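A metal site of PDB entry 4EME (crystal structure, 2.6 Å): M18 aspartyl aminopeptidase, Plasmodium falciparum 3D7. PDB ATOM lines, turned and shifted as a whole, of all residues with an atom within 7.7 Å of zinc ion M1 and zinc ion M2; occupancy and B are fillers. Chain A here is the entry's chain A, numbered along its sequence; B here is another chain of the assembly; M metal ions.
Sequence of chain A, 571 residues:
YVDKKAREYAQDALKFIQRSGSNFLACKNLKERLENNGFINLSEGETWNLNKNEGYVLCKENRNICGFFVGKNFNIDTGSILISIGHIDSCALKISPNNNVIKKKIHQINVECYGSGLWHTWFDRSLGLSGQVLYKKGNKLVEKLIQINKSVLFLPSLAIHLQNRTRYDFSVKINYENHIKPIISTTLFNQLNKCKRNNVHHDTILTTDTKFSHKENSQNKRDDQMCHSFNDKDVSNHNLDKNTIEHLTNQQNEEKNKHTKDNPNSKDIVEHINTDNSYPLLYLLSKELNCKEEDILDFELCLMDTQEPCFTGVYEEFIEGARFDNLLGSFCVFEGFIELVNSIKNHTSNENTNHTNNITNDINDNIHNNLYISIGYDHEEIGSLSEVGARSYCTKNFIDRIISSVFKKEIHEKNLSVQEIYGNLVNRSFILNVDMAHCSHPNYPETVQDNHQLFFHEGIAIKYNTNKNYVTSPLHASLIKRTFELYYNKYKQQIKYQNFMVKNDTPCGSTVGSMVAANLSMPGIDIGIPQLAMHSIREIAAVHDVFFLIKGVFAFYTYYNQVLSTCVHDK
Glu 380 touches zinc ion M2. The nearest printed residue that does not touch zinc ion M2 is His 161 of chain B (4.2 Å).
Zinc ion M2 is bound by OD2 of Asp 325 (2.2 Å), NE2 of His 535 (2.2 Å), OE2 of Glu 381 (2.2 Å) and OE1 of Glu 381 (2.5 Å). Zinc ion M2 has four donor atoms within binding distance.
The side-chain amide nitrogen (ND2) of Asn 326 sits close to the backbone NH (N) of His 87. A ring nitrogen (NE2) of His 535 sits close to a ring nitrogen (NE2) of His 161 of chain B, 3.5 Å away. A ring nitrogen (NE2) of His 87 lies close to the side-chain carboxylate (OE1) of Glu 380 (3.2 Å). The backbone NH (N) of Glu 380 is in hydrogen-bond range of the side-chain carboxylate (OD2) of Asp 89 (3.0 Å). OD1 of Asp 89 is in hydrogen-bond range of ND1 of His 87 (2.8 Å). ND1 of His 535 lies within hydrogen-bond range of SG of Cys 91 (3.3 Å). N of Glu 381 is in hydrogen-bond range of OD2 of Asp 89 (2.8 Å). The backbone NH (N) of Asp 325 sits at hydrogen-bond distance from the side-chain carboxylate (OE1) of Glu 539.
Merely in contact with zinc ion M1: Asn 326 (3.996 Å) and Glu 380 (3.5 Å). Within 4 Å of zinc ion M1: His 87, Asp 325, Asn 326, Glu 380 and Asp 435. The nearest printed residue that does not touch zinc ion M1 is Glu 381 (4.1 Å).
Zinc ion M1 is bound by OD1 of Asp 435 (2.1 Å). Zinc ion M1 is bound by OD1 of Asp 325, at 2.2 Å. NE2 of His 87 is bound to zinc ion M1 (2.3 Å). Zinc ion M1 is bound by the side-chain carboxylate (OD2) of Asp 435.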
ATOM      1  N   GLY A  86     -30.341  -8.535  21.322  1.00  0.00           N
ATOM      2  CA  GLY A  86     -29.453  -7.743  22.148  1.00  0.00           C
ATOM      3  C   GLY A  86     -29.802  -6.296  21.893  1.00  0.00           C
ATOM      4  O   GLY A  86     -30.751  -6.003  21.153  1.00  0.00           O
ATOM      5  N   HIS A  87     -29.067  -5.365  22.495  1.00  0.00           N
ATOM      6  CA  HIS A  87     -29.310  -3.964  22.227  1.00  0.00           C
ATOM      7  C   HIS A  87     -27.989  -3.306  22.086  1.00  0.00           C
ATOM      8  O   HIS A  87     -27.076  -3.635  22.827  1.00  0.00           O
ATOM      9  CB  HIS A  87     -30.259  -3.296  23.239  1.00  0.00           C
ATOM     10  CG  HIS A  87     -29.701  -3.093  24.611  1.00  0.00           C
ATOM     11  ND1 HIS A  87     -28.964  -1.964  24.933  1.00  0.00           N
ATOM     12  CD2 HIS A  87     -29.871  -3.839  25.730  1.00  0.00           C
ATOM     13  CE1 HIS A  87     -28.667  -2.075  26.213  1.00  0.00           C
ATOM     14  NE2 HIS A  87     -29.196  -3.185  26.742  1.00  0.00           N
ATOM     15  N   ASP A  89     -27.242   0.147  22.028  1.00  0.00           N
ATOM     16  CA  ASP A  89     -27.088   1.453  22.705  1.00  0.00           C
ATOM     17  C   ASP A  89     -26.670   1.204  24.154  1.00  0.00           C
ATOM     18  O   ASP A  89     -27.014   0.179  24.743  1.00  0.00           O
ATOM     19  CB  ASP A  89     -28.424   2.212  22.710  1.00  0.00           C
ATOM     20  CG  ASP A  89     -29.521   1.540  23.540  1.00  0.00           C
ATOM     21  OD1 ASP A  89     -29.706   0.310  23.401  1.00  0.00           O
ATOM     22  OD2 ASP A  89     -30.188   2.252  24.336  1.00  0.00           O
ATOM     23  N   SER A  90     -25.959   2.151  24.747  1.00  0.00           N
ATOM     24  CA  SER A  90     -25.573   2.076  26.151  1.00  0.00           C
ATOM     25  C   SER A  90     -25.770   3.459  26.715  1.00  0.00           C
ATOM     26  O   SER A  90     -25.980   4.414  25.963  1.00  0.00           O
ATOM     27  CB  SER A  90     -24.099   1.697  26.291  1.00  0.00           C
ATOM     28  OG  SER A  90     -23.839   0.434  25.712  1.00  0.00           O
ATOM     29  N   CYS A  91     -25.662   3.588  28.040  1.00  0.00           N
ATOM     30  CA  CYS A  91     -25.717   4.863  28.735  1.00  0.00           C
ATOM     31  C   CYS A  91     -24.565   5.687  28.256  1.00  0.00           C
ATOM     32  O   CYS A  91     -23.443   5.188  28.123  1.00  0.00           O
ATOM     33  CB  CYS A  91     -25.650   4.636  30.242  1.00  0.00           C
ATOM     34  SG  CYS A  91     -27.157   3.885  30.906  1.00  0.00           S
ATOM     35  N   GLY A 115     -29.747   7.522  28.956  1.00  0.00           N
ATOM     36  CA  GLY A 115     -29.878   6.318  29.786  1.00  0.00           C
ATOM     37  C   GLY A 115     -29.615   6.637  31.255  1.00  0.00           C
ATOM     38  O   GLY A 115     -29.170   7.742  31.589  1.00  0.00           O
ATOM     39  N   SER A 116     -29.944   5.693  32.149  1.00  0.00           N
ATOM     40  CA  SER A 116     -29.765   5.904  33.585  1.00  0.00           C
ATOM     41  C   SER A 116     -28.352   5.493  34.035  1.00  0.00           C
ATOM     42  O   SER A 116     -28.136   4.472  34.712  1.00  0.00           O
ATOM     43  CB  SER A 116     -30.879   5.226  34.377  1.00  0.00           C
ATOM     44  OG  SER A 116     -30.781   3.823  34.200  1.00  0.00           O
ATOM     45  N   PHE A 324     -20.287  -2.997  28.289  1.00  0.00           N
ATOM     46  CA  PHE A 324     -20.541  -4.460  28.384  1.00  0.00           C
ATOM     47  C   PHE A 324     -22.037  -4.689  28.289  1.00  0.00           C
ATOM     48  O   PHE A 324     -22.481  -5.576  27.572  1.00  0.00           O
ATOM     49  CB  PHE A 324     -19.958  -5.084  29.666  1.00  0.00           C
ATOM     50  CG  PHE A 324     -18.466  -5.358  29.596  1.00  0.00           C
ATOM     51  CD1 PHE A 324     -17.695  -4.880  28.529  1.00  0.00           C
ATOM     52  CD2 PHE A 324     -17.820  -6.070  30.602  1.00  0.00           C
ATOM     53  CE1 PHE A 324     -16.328  -5.122  28.467  1.00  0.00           C
ATOM     54  CE2 PHE A 324     -16.446  -6.301  30.537  1.00  0.00           C
ATOM     55  CZ  PHE A 324     -15.714  -5.839  29.468  1.00  0.00           C
ATOM     56  N   ASP A 325     -22.796  -3.791  28.946  1.00  0.00           N
ATOM     57  CA  ASP A 325     -24.238  -3.678  28.842  1.00  0.00           C
ATOM     58  C   ASP A 325     -24.480  -2.674  27.682  1.00  0.00           C
ATOM     59  O   ASP A 325     -24.280  -1.477  27.873  1.00  0.00           O
ATOM     60  CB  ASP A 325     -24.861  -3.186  30.147  1.00  0.00           C
ATOM     61  CG  ASP A 325     -26.328  -2.840  29.969  1.00  0.00           C
ATOM     62  OD1 ASP A 325     -27.001  -3.515  29.174  1.00  0.00           O
ATOM     63  OD2 ASP A 325     -26.792  -1.877  30.608  1.00  0.00           O
ATOM     64  N   ASN A 326     -24.857  -3.149  26.475  1.00  0.00           N
ATOM     65  CA  ASN A 326     -25.094  -4.567  26.143  1.00  0.00           C
ATOM     66  C   ASN A 326     -24.345  -5.004  24.891  1.00  0.00           C
ATOM     67  O   ASN A 326     -24.813  -5.847  24.132  1.00  0.00           O
ATOM     68  CB  ASN A 326     -26.592  -4.897  26.070  1.00  0.00           C
ATOM     69  CG  ASN A 326     -26.922  -6.358  25.984  1.00  0.00           C
ATOM     70  OD1 ASN A 326     -26.226  -7.214  26.548  1.00  0.00           O
ATOM     71  ND2 ASN A 326     -27.971  -6.691  25.233  1.00  0.00           N
ATOM     72  N   LEU A 327     -23.146  -4.441  24.691  1.00  0.00           N
ATOM     73  CA  LEU A 327     -22.304  -4.791  23.557  1.00  0.00           C
ATOM     74  C   LEU A 327     -21.617  -6.139  23.773  1.00  0.00           C
ATOM     75  O   LEU A 327     -21.260  -6.794  22.788  1.00  0.00           O
ATOM     76  CB  LEU A 327     -21.314  -3.665  23.202  1.00  0.00           C
ATOM     77  CG  LEU A 327     -21.928  -2.354  22.692  1.00  0.00           C
ATOM     78  CD1 LEU A 327     -20.892  -1.501  22.056  1.00  0.00           C
ATOM     79  CD2 LEU A 327     -23.029  -2.619  21.666  1.00  0.00           C
ATOM     80  N   GLU A 380     -32.859   0.855  23.907  1.00  0.00           N
ATOM     81  CA  GLU A 380     -33.251   0.101  25.095  1.00  0.00           C
ATOM     82  C   GLU A 380     -33.079   0.945  26.355  1.00  0.00           C
ATOM     83  O   GLU A 380     -33.979   0.955  27.202  1.00  0.00           O
ATOM     84  CB  GLU A 380     -32.442  -1.194  25.233  1.00  0.00           C
ATOM     85  CG  GLU A 380     -33.010  -2.195  26.236  1.00  0.00           C
ATOM     86  CD  GLU A 380     -32.639  -2.073  27.700  1.00  0.00           C
ATOM     87  OE1 GLU A 380     -31.599  -1.447  28.010  1.00  0.00           O
ATOM     88  OE2 GLU A 380     -33.356  -2.666  28.537  1.00  0.00           O
ATOM     89  N   GLU A 381     -31.960   1.687  26.463  1.00  0.00           N
ATOM     90  CA  GLU A 381     -31.660   2.522  27.630  1.00  0.00           C
ATOM     91  C   GLU A 381     -32.682   3.614  27.962  1.00  0.00           C
ATOM     92  O   GLU A 381     -32.768   4.033  29.122  1.00  0.00           O
ATOM     93  CB  GLU A 381     -30.208   3.049  27.605  1.00  0.00           C
ATOM     94  CG  GLU A 381     -29.148   1.955  27.635  1.00  0.00           C
ATOM     95  CD  GLU A 381     -29.073   0.988  28.810  1.00  0.00           C
ATOM     96  OE1 GLU A 381     -29.907   1.077  29.739  1.00  0.00           O
ATOM     97  OE2 GLU A 381     -28.169   0.130  28.788  1.00  0.00           O
ATOM     98  N   VAL A 434     -31.260 -11.516  25.133  1.00  0.00           N
ATOM     99  CA  VAL A 434     -29.945 -11.467  25.780  1.00  0.00           C
ATOM    100  C   VAL A 434     -29.582 -10.048  26.234  1.00  0.00           C
ATOM    101  O   VAL A 434     -29.492  -9.113  25.423  1.00  0.00           O
ATOM    102  CB  VAL A 434     -28.850 -12.072  24.878  1.00  0.00           C
ATOM    103  CG1 VAL A 434     -27.467 -12.008  25.563  1.00  0.00           C
ATOM    104  CG2 VAL A 434     -29.200 -13.498  24.433  1.00  0.00           C
ATOM    105  N   ASP A 435     -29.377  -9.906  27.540  1.00  0.00           N
ATOM    106  CA  ASP A 435     -28.989  -8.650  28.173  1.00  0.00           C
ATOM    107  C   ASP A 435     -28.264  -8.990  29.437  1.00  0.00           C
ATOM    108  O   ASP A 435     -28.572  -9.995  30.069  1.00  0.00           O
ATOM    109  CB  ASP A 435     -30.219  -7.774  28.494  1.00  0.00           C
ATOM    110  CG  ASP A 435     -29.958  -6.278  28.517  1.00  0.00           C
ATOM    111  OD1 ASP A 435     -28.780  -5.872  28.747  1.00  0.00           O
ATOM    112  OD2 ASP A 435     -30.919  -5.509  28.335  1.00  0.00           O
ATOM    113  N   MET A 436     -27.291  -8.154  29.815  1.00  0.00           N
ATOM    114  CA  MET A 436     -26.463  -8.385  30.998  1.00  0.00           C
ATOM    115  C   MET A 436     -27.233  -8.546  32.303  1.00  0.00           C
ATOM    116  O   MET A 436     -28.321  -7.969  32.452  1.00  0.00           O
ATOM    117  CB  MET A 436     -25.388  -7.304  31.114  1.00  0.00           C
ATOM    118  CG  MET A 436     -24.471  -7.242  29.918  1.00  0.00           C
ATOM    119  SD  MET A 436     -23.630  -8.808  29.593  1.00  0.00           S
ATOM    120  CE  MET A 436     -22.293  -8.684  30.789  1.00  0.00           C
ATOM    121  N   ALA A 437     -26.681  -9.350  33.234  1.00  0.00           N
ATOM    122  CA  ALA A 437     -27.268  -9.645  34.544  1.00  0.00           C
ATOM    123  C   ALA A 437     -26.354  -9.195  35.692  1.00  0.00           C
ATOM    124  O   ALA A 437     -25.152  -8.967  35.480  1.00  0.00           O
ATOM    125  CB  ALA A 437     -27.577 -11.114  34.669  1.00  0.00           C
ATOM    126  N   LYS A 463     -33.008 -15.251  33.833  1.00  0.00           N
ATOM    127  CA  LYS A 463     -33.621 -14.169  34.585  1.00  0.00           C
ATOM    128  C   LYS A 463     -35.130 -14.250  34.690  1.00  0.00           C
ATOM    129  O   LYS A 463     -35.800 -14.193  33.674  1.00  0.00           O
ATOM    130  CB  LYS A 463     -33.192 -12.818  33.974  1.00  0.00           C
ATOM    131  CG  LYS A 463     -31.680 -12.593  33.984  1.00  0.00           C
ATOM    132  CD  LYS A 463     -31.172 -11.857  32.747  1.00  0.00           C
ATOM    133  CE  LYS A 463     -31.570 -10.406  32.725  1.00  0.00           C
ATOM    134  NZ  LYS A 463     -30.673  -9.628  31.836  1.00  0.00           N
ATOM    135  N   SER A 510     -36.160  -3.303  33.373  1.00  0.00           N
ATOM    136  CA  SER A 510     -36.865  -4.094  32.372  1.00  0.00           C
ATOM    137  C   SER A 510     -35.954  -4.390  31.158  1.00  0.00           C
ATOM    138  O   SER A 510     -34.901  -3.755  30.994  1.00  0.00           O
ATOM    139  CB  SER A 510     -38.141  -3.396  31.935  1.00  0.00           C
ATOM    140  OG  SER A 510     -39.122  -3.442  32.967  1.00  0.00           O
ATOM    141  N   THR A 511     -36.365  -5.374  30.324  1.00  0.00           N
ATOM    142  CA  THR A 511     -35.677  -5.777  29.099  1.00  0.00           C
ATOM    143  C   THR A 511     -36.651  -5.621  27.909  1.00  0.00           C
ATOM    144  O   THR A 511     -37.837  -5.389  28.105  1.00  0.00           O
ATOM    145  CB  THR A 511     -35.162  -7.222  29.203  1.00  0.00           C
ATOM    146  OG1 THR A 511     -36.269  -8.108  29.385  1.00  0.00           O
ATOM    147  CG2 THR A 511     -34.127  -7.418  30.306  1.00  0.00           C
ATOM    148  N   VAL A 512     -36.150  -5.767  26.697  1.00  0.00           N
ATOM    149  CA  VAL A 512     -36.981  -5.680  25.501  1.00  0.00           C
ATOM    150  C   VAL A 512     -37.760  -6.975  25.216  1.00  0.00           C
ATOM    151  O   VAL A 512     -38.556  -7.001  24.293  1.00  0.00           O
ATOM    152  CB  VAL A 512     -36.175  -5.222  24.277  1.00  0.00           C
ATOM    153  CG1 VAL A 512     -35.642  -3.820  24.479  1.00  0.00           C
ATOM    154  CG2 VAL A 512     -35.050  -6.187  23.933  1.00  0.00           C
ATOM    155  N   GLN A 531     -22.405  -9.626  35.527  1.00  0.00           N
ATOM    156  CA  GLN A 531     -21.407  -8.555  35.556  1.00  0.00           C
ATOM    157  C   GLN A 531     -21.602  -7.726  36.819  1.00  0.00           C
ATOM    158  O   GLN A 531     -22.645  -7.838  37.470  1.00  0.00           O
ATOM    159  CB  GLN A 531     -21.498  -7.658  34.301  1.00  0.00           C
ATOM    160  CG  GLN A 531     -22.783  -6.847  34.230  1.00  0.00           C
ATOM    161  CD  GLN A 531     -22.620  -5.524  33.545  1.00  0.00           C
ATOM    162  OE1 GLN A 531     -23.169  -5.290  32.487  1.00  0.00           O
ATOM    163  NE2 GLN A 531     -21.930  -4.596  34.184  1.00  0.00           N
ATOM    164  N   MET A 534     -23.111  -2.270  36.593  1.00  0.00           N
ATOM    165  CA  MET A 534     -23.919  -1.966  35.408  1.00  0.00           C
ATOM    166  C   MET A 534     -24.290  -0.502  35.379  1.00  0.00           C
ATOM    167  O   MET A 534     -24.750   0.038  36.385  1.00  0.00           O
ATOM    168  CB  MET A 534     -25.167  -2.857  35.329  1.00  0.00           C
ATOM    169  CG  MET A 534     -25.627  -3.111  33.896  1.00  0.00           C
ATOM    170  SD  MET A 534     -27.072  -4.210  33.763  1.00  0.00           S
ATOM    171  CE  MET A 534     -26.351  -5.763  34.334  1.00  0.00           C
ATOM    172  N   HIS A 535     -24.074   0.135  34.204  1.00  0.00           N
ATOM    173  CA  HIS A 535     -24.328   1.549  33.886  1.00  0.00           C
ATOM    174  C   HIS A 535     -23.167   2.510  34.206  1.00  0.00           C
ATOM    175  O   HIS A 535     -23.296   3.729  34.084  1.00  0.00           O
ATOM    176  CB  HIS A 535     -25.732   2.042  34.313  1.00  0.00           C
ATOM    177  CG  HIS A 535     -26.826   1.423  33.501  1.00  0.00           C
ATOM    178  ND1 HIS A 535     -28.077   2.006  33.442  1.00  0.00           N
ATOM    179  CD2 HIS A 535     -26.797   0.337  32.696  1.00  0.00           C
ATOM    180  CE1 HIS A 535     -28.780   1.234  32.632  1.00  0.00           C
ATOM    181  NE2 HIS A 535     -28.045   0.225  32.146  1.00  0.00           N
ATOM    182  N   GLU A 539     -17.434  -1.360  33.317  1.00  0.00           N
ATOM    183  CA  GLU A 539     -18.071  -2.508  33.950  1.00  0.00           C
ATOM    184  C   GLU A 539     -17.117  -3.702  33.949  1.00  0.00           C
ATOM    185  O   GLU A 539     -16.050  -3.612  33.357  1.00  0.00           O
ATOM    186  CB  GLU A 539     -19.382  -2.799  33.208  1.00  0.00           C
ATOM    187  CG  GLU A 539     -20.262  -1.559  33.038  1.00  0.00           C
ATOM    188  CD  GLU A 539     -21.405  -1.695  32.044  1.00  0.00           C
ATOM    189  OE1 GLU A 539     -21.282  -2.476  31.084  1.00  0.00           O
ATOM    190  OE2 GLU A 539     -22.438  -1.003  32.241  1.00  0.00           O
ATOM    191  N   ILE B 160     -26.681   0.572  39.124  1.00  0.00           N
ATOM    192  CA  ILE B 160     -27.688   1.593  39.431  1.00  0.00           C
ATOM    193  C   ILE B 160     -29.084   0.963  39.683  1.00  0.00           C
ATOM    194  O   ILE B 160     -29.904   1.515  40.422  1.00  0.00           O
ATOM    195  CB  ILE B 160     -27.727   2.705  38.335  1.00  0.00           C
ATOM    196  CG1 ILE B 160     -28.497   3.973  38.827  1.00  0.00           C
ATOM    197  CG2 ILE B 160     -28.234   2.168  36.994  1.00  0.00           C
ATOM    198  CD1 ILE B 160     -28.217   5.253  38.137  1.00  0.00           C
ATOM    199  N   HIS B 161     -29.315  -0.205  39.075  1.00  0.00           N
ATOM    200  CA  HIS B 161     -30.560  -0.970  39.154  1.00  0.00           C
ATOM    201  C   HIS B 161     -30.803  -1.444  40.580  1.00  0.00           C
ATOM    202  O   HIS B 161     -31.954  -1.533  41.002  1.00  0.00           O
ATOM    203  CB  HIS B 161     -30.493  -2.165  38.202  1.00  0.00           C
ATOM    204  CG  HIS B 161     -29.986  -1.827  36.829  1.00  0.00           C
ATOM    205  ND1 HIS B 161     -28.670  -1.450  36.620  1.00  0.00           N
ATOM    206  CD2 HIS B 161     -30.625  -1.852  35.644  1.00  0.00           C
ATOM    207  CE1 HIS B 161     -28.563  -1.238  35.320  1.00  0.00           C
ATOM    208  NE2 HIS B 161     -29.717  -1.475  34.688  1.00  0.00           N
HETATM  209 ZN    ZN M   1     -29.160  -3.820  28.936  1.00  0.00          ZN
HETATM  210 ZN    ZN M   2     -28.812  -1.066  30.562  1.00  0.00          ZN
